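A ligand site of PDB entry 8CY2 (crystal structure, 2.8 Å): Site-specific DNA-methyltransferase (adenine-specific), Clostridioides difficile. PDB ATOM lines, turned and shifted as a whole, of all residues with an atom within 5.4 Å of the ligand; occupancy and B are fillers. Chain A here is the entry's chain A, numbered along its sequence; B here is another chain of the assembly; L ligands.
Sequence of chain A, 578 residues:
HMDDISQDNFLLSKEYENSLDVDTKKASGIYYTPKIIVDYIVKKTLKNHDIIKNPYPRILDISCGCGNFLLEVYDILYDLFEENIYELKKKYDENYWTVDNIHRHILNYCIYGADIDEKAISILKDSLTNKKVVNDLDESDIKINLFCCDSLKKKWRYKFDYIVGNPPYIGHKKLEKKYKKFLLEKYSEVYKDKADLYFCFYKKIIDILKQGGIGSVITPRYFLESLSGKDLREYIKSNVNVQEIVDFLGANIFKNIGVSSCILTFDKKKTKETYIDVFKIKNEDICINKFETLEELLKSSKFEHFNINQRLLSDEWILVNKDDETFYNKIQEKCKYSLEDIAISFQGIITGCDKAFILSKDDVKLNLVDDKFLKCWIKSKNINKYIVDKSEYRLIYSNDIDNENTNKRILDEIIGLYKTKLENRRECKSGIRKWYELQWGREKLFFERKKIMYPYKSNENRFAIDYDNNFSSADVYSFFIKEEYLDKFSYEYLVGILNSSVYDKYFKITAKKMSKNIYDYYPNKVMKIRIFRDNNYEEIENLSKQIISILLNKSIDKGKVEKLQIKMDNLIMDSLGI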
ATOM      1  N   GLY A  29      -7.152 -34.873  13.955  1.00  0.00           N
ATOM      2  CA  GLY A  29      -7.002 -33.827  14.964  1.00  0.00           C
ATOM      3  C   GLY A  29      -7.816 -32.570  14.694  1.00  0.00           C
ATOM      4  O   GLY A  29      -8.018 -31.754  15.604  1.00  0.00           O
ATOM      5  N   ILE A  30      -8.296 -32.411  13.456  1.00  0.00           N
ATOM      6  CA  ILE A  30      -9.074 -31.252  13.029  1.00  0.00           C
ATOM      7  C   ILE A  30     -10.450 -31.717  12.570  1.00  0.00           C
ATOM      8  O   ILE A  30     -10.571 -32.737  11.873  1.00  0.00           O
ATOM      9  CB  ILE A  30      -8.358 -30.465  11.916  1.00  0.00           C
ATOM     10  N   TYR A  31     -11.477 -30.960  12.957  1.00  0.00           N
ATOM     11  CA  TYR A  31     -12.863 -31.272  12.628  1.00  0.00           C
ATOM     12  C   TYR A  31     -13.502 -30.072  11.932  1.00  0.00           C
ATOM     13  O   TYR A  31     -13.454 -28.951  12.463  1.00  0.00           O
ATOM     14  CB  TYR A  31     -13.667 -31.635  13.887  1.00  0.00           C
ATOM     15  CG  TYR A  31     -13.056 -32.767  14.675  1.00  0.00           C
ATOM     16  CD1 TYR A  31     -12.107 -32.518  15.653  1.00  0.00           C
ATOM     17  CD2 TYR A  31     -13.431 -34.089  14.443  1.00  0.00           C
ATOM     18  CE1 TYR A  31     -11.533 -33.552  16.377  1.00  0.00           C
ATOM     19  CE2 TYR A  31     -12.865 -35.128  15.165  1.00  0.00           C
ATOM     20  CZ  TYR A  31     -11.920 -34.853  16.124  1.00  0.00           C
ATOM     21  OH  TYR A  31     -11.363 -35.882  16.852  1.00  0.00           O
ATOM     22  N   ILE A  62     -10.682 -19.403  19.819  1.00  0.00           N
ATOM     23  CA  ILE A  62      -9.555 -19.980  20.544  1.00  0.00           C
ATOM     24  C   ILE A  62      -9.247 -21.405  20.132  1.00  0.00           C
ATOM     25  O   ILE A  62      -8.353 -22.027  20.716  1.00  0.00           O
ATOM     26  CB  ILE A  62      -9.767 -19.947  22.066  1.00  0.00           C
ATOM     27  CG1 ILE A  62     -11.136 -20.473  22.454  1.00  0.00           C
ATOM     28  CG2 ILE A  62      -9.602 -18.543  22.594  1.00  0.00           C
ATOM     29  CD1 ILE A  62     -11.298 -20.602  23.953  1.00  0.00           C
ATOM     30  N   SER A  63      -9.973 -21.957  19.167  1.00  0.00           N
ATOM     31  CA  SER A  63      -9.603 -23.235  18.560  1.00  0.00           C
ATOM     32  C   SER A  63      -9.813 -23.144  17.055  1.00  0.00           C
ATOM     33  O   SER A  63     -10.456 -23.984  16.433  1.00  0.00           O
ATOM     34  CB  SER A  63     -10.392 -24.391  19.186  1.00  0.00           C
ATOM     35  OG  SER A  63     -11.780 -24.097  19.193  1.00  0.00           O
ATOM     36  N   CYS A  64      -9.265 -22.076  16.463  1.00  0.00           N
ATOM     37  CA  CYS A  64      -9.682 -21.657  15.119  1.00  0.00           C
ATOM     38  C   CYS A  64      -9.343 -22.690  14.046  1.00  0.00           C
ATOM     39  O   CYS A  64     -10.004 -22.719  13.002  1.00  0.00           O
ATOM     40  CB  CYS A  64      -9.038 -20.318  14.774  1.00  0.00           C
ATOM     41  SG  CYS A  64      -7.252 -20.315  14.985  1.00  0.00           S
ATOM     42  N   GLY A  65      -8.334 -23.525  14.281  1.00  0.00           N
ATOM     43  CA  GLY A  65      -8.021 -24.537  13.280  1.00  0.00           C
ATOM     44  C   GLY A  65      -7.594 -23.911  11.973  1.00  0.00           C
ATOM     45  O   GLY A  65      -6.771 -22.982  11.941  1.00  0.00           O
ATOM     46  N   ALA A 114      -6.500 -18.506  17.913  1.00  0.00           N
ATOM     47  CA  ALA A 114      -5.574 -19.317  18.695  1.00  0.00           C
ATOM     48  C   ALA A 114      -5.763 -20.777  18.340  1.00  0.00           C
ATOM     49  O   ALA A 114      -6.898 -21.247  18.192  1.00  0.00           O
ATOM     50  CB  ALA A 114      -5.782 -19.117  20.206  1.00  0.00           C
ATOM     51  N   ASP A 115      -4.652 -21.496  18.194  1.00  0.00           N
ATOM     52  CA  ASP A 115      -4.713 -22.933  18.022  1.00  0.00           C
ATOM     53  C   ASP A 115      -3.353 -23.512  18.327  1.00  0.00           C
ATOM     54  O   ASP A 115      -2.324 -22.828  18.220  1.00  0.00           O
ATOM     55  CB  ASP A 115      -5.169 -23.329  16.618  1.00  0.00           C
ATOM     56  CG  ASP A 115      -5.754 -24.730  16.572  1.00  0.00           C
ATOM     57  OD1 ASP A 115      -5.054 -25.678  16.977  1.00  0.00           O
ATOM     58  OD2 ASP A 115      -6.926 -24.870  16.153  1.00  0.00           O
ATOM     59  N   ILE A 116      -3.341 -24.796  18.703  1.00  0.00           N
ATOM     60  CA  ILE A 116      -2.092 -25.458  19.067  1.00  0.00           C
ATOM     61  C   ILE A 116      -1.387 -26.074  17.858  1.00  0.00           C
ATOM     62  O   ILE A 116      -0.212 -26.445  17.969  1.00  0.00           O
ATOM     63  CB  ILE A 116      -2.382 -26.495  20.166  1.00  0.00           C
ATOM     64  CG1 ILE A 116      -1.102 -26.832  20.935  1.00  0.00           C
ATOM     65  CG2 ILE A 116      -3.048 -27.736  19.582  1.00  0.00           C
ATOM     66  CD1 ILE A 116      -1.343 -27.526  22.254  1.00  0.00           C
ATOM     67  N   ASP A 117      -2.062 -26.179  16.709  1.00  0.00           N
ATOM     68  CA  ASP A 117      -1.486 -26.758  15.509  1.00  0.00           C
ATOM     69  C   ASP A 117      -0.804 -25.665  14.672  1.00  0.00           C
ATOM     70  O   ASP A 117      -1.471 -24.770  14.151  1.00  0.00           O
ATOM     71  CB  ASP A 117      -2.566 -27.456  14.684  1.00  0.00           C
ATOM     72  CG  ASP A 117      -2.028 -28.145  13.445  1.00  0.00           C
ATOM     73  OD1 ASP A 117      -0.790 -28.351  13.346  1.00  0.00           O
ATOM     74  OD2 ASP A 117      -2.830 -28.490  12.548  1.00  0.00           O
ATOM     75  N   CYS A 149      -0.543 -21.663  20.476  1.00  0.00           N
ATOM     76  CA  CYS A 149      -0.362 -21.934  21.899  1.00  0.00           C
ATOM     77  C   CYS A 149      -1.522 -22.784  22.401  1.00  0.00           C
ATOM     78  O   CYS A 149      -2.480 -23.060  21.681  1.00  0.00           O
ATOM     79  CB  CYS A 149      -0.286 -20.640  22.701  1.00  0.00           C
ATOM     80  SG  CYS A 149      -1.878 -19.780  22.772  1.00  0.00           S
ATOM     81  N   ASP A 150      -1.401 -23.191  23.664  1.00  0.00           N
ATOM     82  CA  ASP A 150      -2.499 -23.818  24.391  1.00  0.00           C
ATOM     83  C   ASP A 150      -3.414 -22.723  24.934  1.00  0.00           C
ATOM     84  O   ASP A 150      -3.020 -21.980  25.832  1.00  0.00           O
ATOM     85  CB  ASP A 150      -1.942 -24.669  25.532  1.00  0.00           C
ATOM     86  CG  ASP A 150      -3.016 -25.463  26.260  1.00  0.00           C
ATOM     87  OD1 ASP A 150      -4.213 -25.138  26.109  1.00  0.00           O
ATOM     88  OD2 ASP A 150      -2.643 -26.411  26.973  1.00  0.00           O
ATOM     89  N   SER A 151      -4.633 -22.640  24.402  1.00  0.00           N
ATOM     90  CA  SER A 151      -5.538 -21.580  24.816  1.00  0.00           C
ATOM     91  C   SER A 151      -5.862 -21.640  26.301  1.00  0.00           C
ATOM     92  O   SER A 151      -6.208 -20.612  26.899  1.00  0.00           O
ATOM     93  CB  SER A 151      -6.829 -21.641  24.000  1.00  0.00           C
ATOM     94  OG  SER A 151      -6.545 -21.566  22.617  1.00  0.00           O
ATOM     95  N   LEU A 152      -5.767 -22.819  26.921  1.00  0.00           N
ATOM     96  CA  LEU A 152      -6.051 -22.952  28.342  1.00  0.00           C
ATOM     97  C   LEU A 152      -4.883 -22.556  29.229  1.00  0.00           C
ATOM     98  O   LEU A 152      -5.070 -22.420  30.445  1.00  0.00           O
ATOM     99  CB  LEU A 152      -6.466 -24.392  28.658  1.00  0.00           C
ATOM    100  CG  LEU A 152      -7.667 -24.902  27.869  1.00  0.00           C
ATOM    101  CD1 LEU A 152      -8.082 -26.253  28.402  1.00  0.00           C
ATOM    102  CD2 LEU A 152      -8.823 -23.905  27.953  1.00  0.00           C
ATOM    103  N   ASN A 166     -15.533 -23.778  17.652  1.00  0.00           N
ATOM    104  CA  ASN A 166     -15.853 -25.181  17.915  1.00  0.00           C
ATOM    105  C   ASN A 166     -14.682 -25.780  18.696  1.00  0.00           C
ATOM    106  O   ASN A 166     -13.669 -26.165  18.089  1.00  0.00           O
ATOM    107  CB  ASN A 166     -16.101 -25.932  16.621  1.00  0.00           C
ATOM    108  CG  ASN A 166     -16.310 -27.423  16.830  1.00  0.00           C
ATOM    109  OD1 ASN A 166     -16.793 -27.863  17.865  1.00  0.00           O
ATOM    110  ND2 ASN A 166     -15.960 -28.211  15.813  1.00  0.00           N
ATOM    111  N   PRO A 167     -14.782 -25.870  20.019  1.00  0.00           N
ATOM    112  CA  PRO A 167     -13.644 -26.282  20.845  1.00  0.00           C
ATOM    113  C   PRO A 167     -13.370 -27.771  20.703  1.00  0.00           C
ATOM    114  O   PRO A 167     -14.205 -28.508  20.168  1.00  0.00           O
ATOM    115  CB  PRO A 167     -14.101 -25.929  22.264  1.00  0.00           C
ATOM    116  CG  PRO A 167     -15.580 -26.142  22.214  1.00  0.00           C
ATOM    117  CD  PRO A 167     -16.002 -25.673  20.822  1.00  0.00           C
ATOM    118  N   PRO A 168     -12.221 -28.256  21.178  1.00  0.00           N
ATOM    119  CA  PRO A 168     -11.948 -29.695  21.132  1.00  0.00           C
ATOM    120  C   PRO A 168     -12.655 -30.458  22.230  1.00  0.00           C
ATOM    121  O   PRO A 168     -12.818 -29.962  23.354  1.00  0.00           O
ATOM    122  CB  PRO A 168     -10.421 -29.761  21.311  1.00  0.00           C
ATOM    123  CG  PRO A 168     -10.115 -28.582  22.153  1.00  0.00           C
ATOM    124  CD  PRO A 168     -11.057 -27.499  21.686  1.00  0.00           C
ATOM    125  N   ILE A 170     -12.400 -33.836  24.409  1.00  0.00           N
ATOM    126  CA  ILE A 170     -11.616 -34.976  24.867  1.00  0.00           C
ATOM    127  C   ILE A 170     -12.225 -35.475  26.170  1.00  0.00           C
ATOM    128  O   ILE A 170     -12.305 -34.723  27.154  1.00  0.00           O
ATOM    129  CB  ILE A 170     -10.130 -34.637  25.071  1.00  0.00           C
ATOM    130  CG1 ILE A 170      -9.616 -33.700  23.974  1.00  0.00           C
ATOM    131  CG2 ILE A 170      -9.315 -35.924  25.085  1.00  0.00           C
ATOM    132  CD1 ILE A 170      -9.320 -34.382  22.653  1.00  0.00           C
ATOM    133  N   LYS A 174      -9.341 -40.466  26.967  1.00  0.00           N
ATOM    134  CA  LYS A 174      -8.412 -40.049  25.927  1.00  0.00           C
ATOM    135  C   LYS A 174      -7.580 -38.834  26.305  1.00  0.00           C
ATOM    136  O   LYS A 174      -6.803 -38.359  25.467  1.00  0.00           O
ATOM    137  CB  LYS A 174      -9.182 -39.775  24.626  1.00  0.00           C
ATOM    138  CG  LYS A 174     -10.080 -40.941  24.199  1.00  0.00           C
ATOM    139  CD  LYS A 174     -10.908 -40.619  22.962  1.00  0.00           C
ATOM    140  CE  LYS A 174     -11.854 -41.769  22.602  1.00  0.00           C
ATOM    141  NZ  LYS A 174     -12.649 -41.522  21.354  1.00  0.00           N
ATOM    142  N   LEU A 175      -7.718 -38.325  27.522  1.00  0.00           N
ATOM    143  CA  LEU A 175      -6.952 -37.170  27.969  1.00  0.00           C
ATOM    144  C   LEU A 175      -5.761 -37.622  28.804  1.00  0.00           C
ATOM    145  O   LEU A 175      -5.884 -38.508  29.658  1.00  0.00           O
ATOM    146  CB  LEU A 175      -7.838 -36.225  28.786  1.00  0.00           C
ATOM    147  CG  LEU A 175      -7.320 -34.805  29.000  1.00  0.00           C
ATOM    148  CD1 LEU A 175      -6.867 -34.210  27.678  1.00  0.00           C
ATOM    149  CD2 LEU A 175      -8.418 -33.952  29.610  1.00  0.00           C
ATOM    150  N   GLU A 176      -4.606 -37.008  28.554  1.00  0.00           N
ATOM    151  CA  GLU A 176      -3.368 -37.404  29.236  1.00  0.00           C
ATOM    152  C   GLU A 176      -3.411 -37.012  30.710  1.00  0.00           C
ATOM    153  O   GLU A 176      -3.919 -35.952  31.073  1.00  0.00           O
ATOM    154  CB  GLU A 176      -2.165 -36.773  28.536  1.00  0.00           C
ATOM    155  CG  GLU A 176      -0.874 -36.652  29.391  1.00  0.00           C
ATOM    156  CD  GLU A 176      -0.227 -37.997  29.778  1.00  0.00           C
ATOM    157  OE1 GLU A 176      -0.904 -39.050  29.788  1.00  0.00           O
ATOM    158  OE2 GLU A 176       0.984 -37.990  30.094  1.00  0.00           O
ATOM    159  N   TYR A 179      -1.810 -33.556  31.881  1.00  0.00           N
ATOM    160  CA  TYR A 179      -2.687 -32.445  31.585  1.00  0.00           C
ATOM    161  C   TYR A 179      -3.934 -32.464  32.461  1.00  0.00           C
ATOM    162  O   TYR A 179      -4.455 -31.403  32.819  1.00  0.00           O
ATOM    163  CB  TYR A 179      -3.063 -32.491  30.101  1.00  0.00           C
ATOM    164  CG  TYR A 179      -3.538 -31.160  29.573  1.00  0.00           C
ATOM    165  CD1 TYR A 179      -2.625 -30.213  29.139  1.00  0.00           C
ATOM    166  CD2 TYR A 179      -4.882 -30.863  29.530  1.00  0.00           C
ATOM    167  CE1 TYR A 179      -3.052 -28.995  28.683  1.00  0.00           C
ATOM    168  CE2 TYR A 179      -5.319 -29.646  29.059  1.00  0.00           C
ATOM    169  CZ  TYR A 179      -4.399 -28.712  28.643  1.00  0.00           C
ATOM    170  OH  TYR A 179      -4.828 -27.490  28.173  1.00  0.00           O
ATOM    171  N   LEU A 197     -12.875 -31.813  28.409  1.00  0.00           N
ATOM    172  CA  LEU A 197     -12.028 -30.646  28.154  1.00  0.00           C
ATOM    173  C   LEU A 197     -12.853 -29.437  27.707  1.00  0.00           C
ATOM    174  O   LEU A 197     -12.537 -28.284  28.064  1.00  0.00           O
ATOM    175  CB  LEU A 197     -11.009 -31.022  27.084  1.00  0.00           C
ATOM    176  CG  LEU A 197      -9.981 -29.979  26.666  1.00  0.00           C
ATOM    177  CD1 LEU A 197      -9.101 -29.631  27.845  1.00  0.00           C
ATOM    178  CD2 LEU A 197      -9.161 -30.506  25.508  1.00  0.00           C
ATOM    179  N   PHE A 201     -12.932 -25.190  28.107  1.00  0.00           N
ATOM    180  CA  PHE A 201     -13.044 -24.166  27.062  1.00  0.00           C
ATOM    181  C   PHE A 201     -14.243 -23.251  27.318  1.00  0.00           C
ATOM    182  O   PHE A 201     -14.154 -22.033  27.087  1.00  0.00           O
ATOM    183  CB  PHE A 201     -13.110 -24.803  25.682  1.00  0.00           C
ATOM    184  CG  PHE A 201     -11.772 -25.091  25.102  1.00  0.00           C
ATOM    185  CD1 PHE A 201     -11.055 -26.201  25.526  1.00  0.00           C
ATOM    186  CD2 PHE A 201     -11.202 -24.234  24.181  1.00  0.00           C
ATOM    187  CE1 PHE A 201      -9.805 -26.469  25.019  1.00  0.00           C
ATOM    188  CE2 PHE A 201      -9.948 -24.505  23.664  1.00  0.00           C
ATOM    189  CZ  PHE A 201      -9.247 -25.627  24.085  1.00  0.00           C
ATOM    190  P    DA B   8     -16.085 -39.570  23.124  1.00  0.00           P
ATOM    191  OP1  DA B   8     -15.215 -40.644  22.602  1.00  0.00           O
ATOM    192  OP2  DA B   8     -15.534 -38.601  24.105  1.00  0.00           O
ATOM    193  O5'  DA B   8     -16.682 -38.765  21.893  1.00  0.00           O
ATOM    194  C5'  DA B   8     -15.989 -37.655  21.375  1.00  0.00           C
ATOM    195  C4'  DA B   8     -16.203 -37.545  19.886  1.00  0.00           C
ATOM    196  O4'  DA B   8     -16.168 -36.151  19.486  1.00  0.00           O
ATOM    197  C3'  DA B   8     -15.151 -38.252  19.041  1.00  0.00           C
ATOM    198  O3'  DA B   8     -15.779 -38.833  17.923  1.00  0.00           O
ATOM    199  C2'  DA B   8     -14.238 -37.104  18.618  1.00  0.00           C
ATOM    200  C1'  DA B   8     -15.261 -36.002  18.413  1.00  0.00           C
ATOM    201  N9   DA B   8     -14.723 -34.652  18.445  1.00  0.00           N
ATOM    202  C8   DA B   8     -13.672 -34.201  19.184  1.00  0.00           C
ATOM    203  N7   DA B   8     -13.420 -32.916  19.027  1.00  0.00           N
ATOM    204  C5   DA B   8     -14.392 -32.509  18.132  1.00  0.00           C
ATOM    205  C6   DA B   8     -14.675 -31.253  17.542  1.00  0.00           C
ATOM    206  N6   DA B   8     -13.983 -30.143  17.797  1.00  0.00           N
ATOM    207  N1   DA B   8     -15.715 -31.185  16.683  1.00  0.00           N
ATOM    208  C2   DA B   8     -16.407 -32.296  16.428  1.00  0.00           C
ATOM    209  N3   DA B   8     -16.239 -33.525  16.913  1.00  0.00           N
ATOM    210  C4   DA B   8     -15.198 -33.558  17.762  1.00  0.00           C
HETATM  211  C1  LIG L   1      -9.262 -27.838  17.253  1.00  0.00           C
HETATM  212  C2  LIG L   1      -6.956 -28.383  17.613  1.00  0.00           C
HETATM  213  O1  LIG L   1      -5.625 -28.101  17.180  1.00  0.00           O
HETATM  214  N1  LIG L   1      -6.973 -27.470  19.944  1.00  0.00           N
HETATM  215  C3  LIG L   1      -7.998 -28.256  16.495  1.00  0.00           C
HETATM  216  O2  LIG L   1      -7.664 -27.287  15.509  1.00  0.00           O
HETATM  217  C4  LIG L   1      -5.531 -28.144  24.696  1.00  0.00           C
HETATM  218  C5  LIG L   1      -4.147 -28.742  24.563  1.00  0.00           C
HETATM  219  C6  LIG L   1      -4.113 -30.232  24.817  1.00  0.00           C
HETATM  220  C7  LIG L   1      -2.978 -30.833  25.364  1.00  0.00           C
HETATM  221  C8  LIG L   1      -2.944 -32.200  25.606  1.00  0.00           C
HETATM  222  C9  LIG L   1      -4.041 -33.006  25.292  1.00  0.00           C
HETATM  223  C10 LIG L   1      -5.173 -32.392  24.742  1.00  0.00           C
HETATM  224  C11 LIG L   1      -5.201 -31.032  24.504  1.00  0.00           C
HETATM  225  C12 LIG L   1     -10.273 -28.941  17.462  1.00  0.00           C
HETATM  226  C13 LIG L   1      -7.423 -27.287  18.566  1.00  0.00           C
HETATM  227  C14 LIG L   1      -6.950 -28.627  20.674  1.00  0.00           C
HETATM  228  C15 LIG L   1      -6.276 -27.121  22.003  1.00  0.00           C
HETATM  229  C16 LIG L   1      -6.530 -26.481  20.802  1.00  0.00           C
HETATM  230  C17 LIG L   1      -5.964 -24.510  21.607  1.00  0.00           C
HETATM  231  C18 LIG L   1      -5.839 -26.287  23.068  1.00  0.00           C
HETATM  232  N2  LIG L   1      -6.549 -28.474  21.906  1.00  0.00           N
HETATM  233  N3  LIG L   1      -6.392 -25.185  20.534  1.00  0.00           N
HETATM  234  N4  LIG L   1      -5.695 -24.973  22.830  1.00  0.00           N
HETATM  235  N5  LIG L   1      -5.525 -26.744  24.295  1.00  0.00           N
HETATM  236  N6  LIG L   1      -4.012 -34.365  25.529  1.00  0.00           N
HETATM  237  O3  LIG L   1     -11.426 -28.730  16.642  1.00  0.00           O
HETATM  238  O4  LIG L   1      -8.829 -27.335  18.542  1.00  0.00           O
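OD1 of Asp 115 sits at hydrogen-bond distance from O1 of the ligand (2.5 Å). OD1 of Asp 150 is in hydrogen-bond range of N5 of the ligand (2.8 Å). N of Ser 151 is in hydrogen-bond range of N4 of the ligand, at 3.0 Å. N6 of DA 8 of chain B sits at hydrogen-bond distance from an oxygen (O3) of the ligand, 3.1 Å away.
N of Gly 65 lies within hydrogen-bond range of OD2 of Asp 115 (2.7 Å). N of Cys 149 sits at hydrogen-bond distance from O of Asp 115, 3.1 Å away. The side-chain carboxylate (OD1) of Asp 115 sits at hydrogen-bond distance from the backbone NH (N) of Asp 117, 3.0 Å away. OD1 of Asp 150 is in hydrogen-bond range of N of Leu 152. The side-chain hydroxyl (OG) of Ser 151 is in hydrogen-bond range of the backbone carbonyl oxygen (O) of Ile 62, at 2.7 Å. N1 of DA 8 of chain B is in hydrogen-bond range of ND2 of Asn 166 (3.1 Å). The backbone carbonyl oxygen (O) of Asn 166 lies within hydrogen-bond range of the side-chain hydroxyl (OG) of Ser 63 (3.0 Å). N of Ser 63 is in hydrogen-bond range of O of Ala 114 (3.3 Å).
Gly 29 touches the ligand. Tyr 31 touches the ligand. Ile 62 touches the ligand. Ser 63 touches the ligand. Gly 65 touches the ligand. Ile 116 touches the ligand (CG2 to O1, 3.5 Å). Cys 149 touches the ligand (O to C17, 3.8 Å). Asn 166 touches the ligand (O to O3, 3.7 Å). CG of Pro 168 touches C14 of the ligand, 3.5 Å away. Leu 175 touches the ligand. Tyr 179 touches the ligand (OH to C4, 3.6 Å). Phe 201 touches the ligand (CZ to C18, 3.6 Å). Within 4 Å of the ligand: Gly 29, Tyr 31, Ile 62, Ser 63, Gly 65, Asp 115, Ile 116, Cys 149, Asp 150, Ser 151, Asn 166, Pro 168, Leu 175, Tyr 179, Phe 201 and DA 8 of chain B. Along chain A the residues within 4 Å of the ligand span positions 29 to 201.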
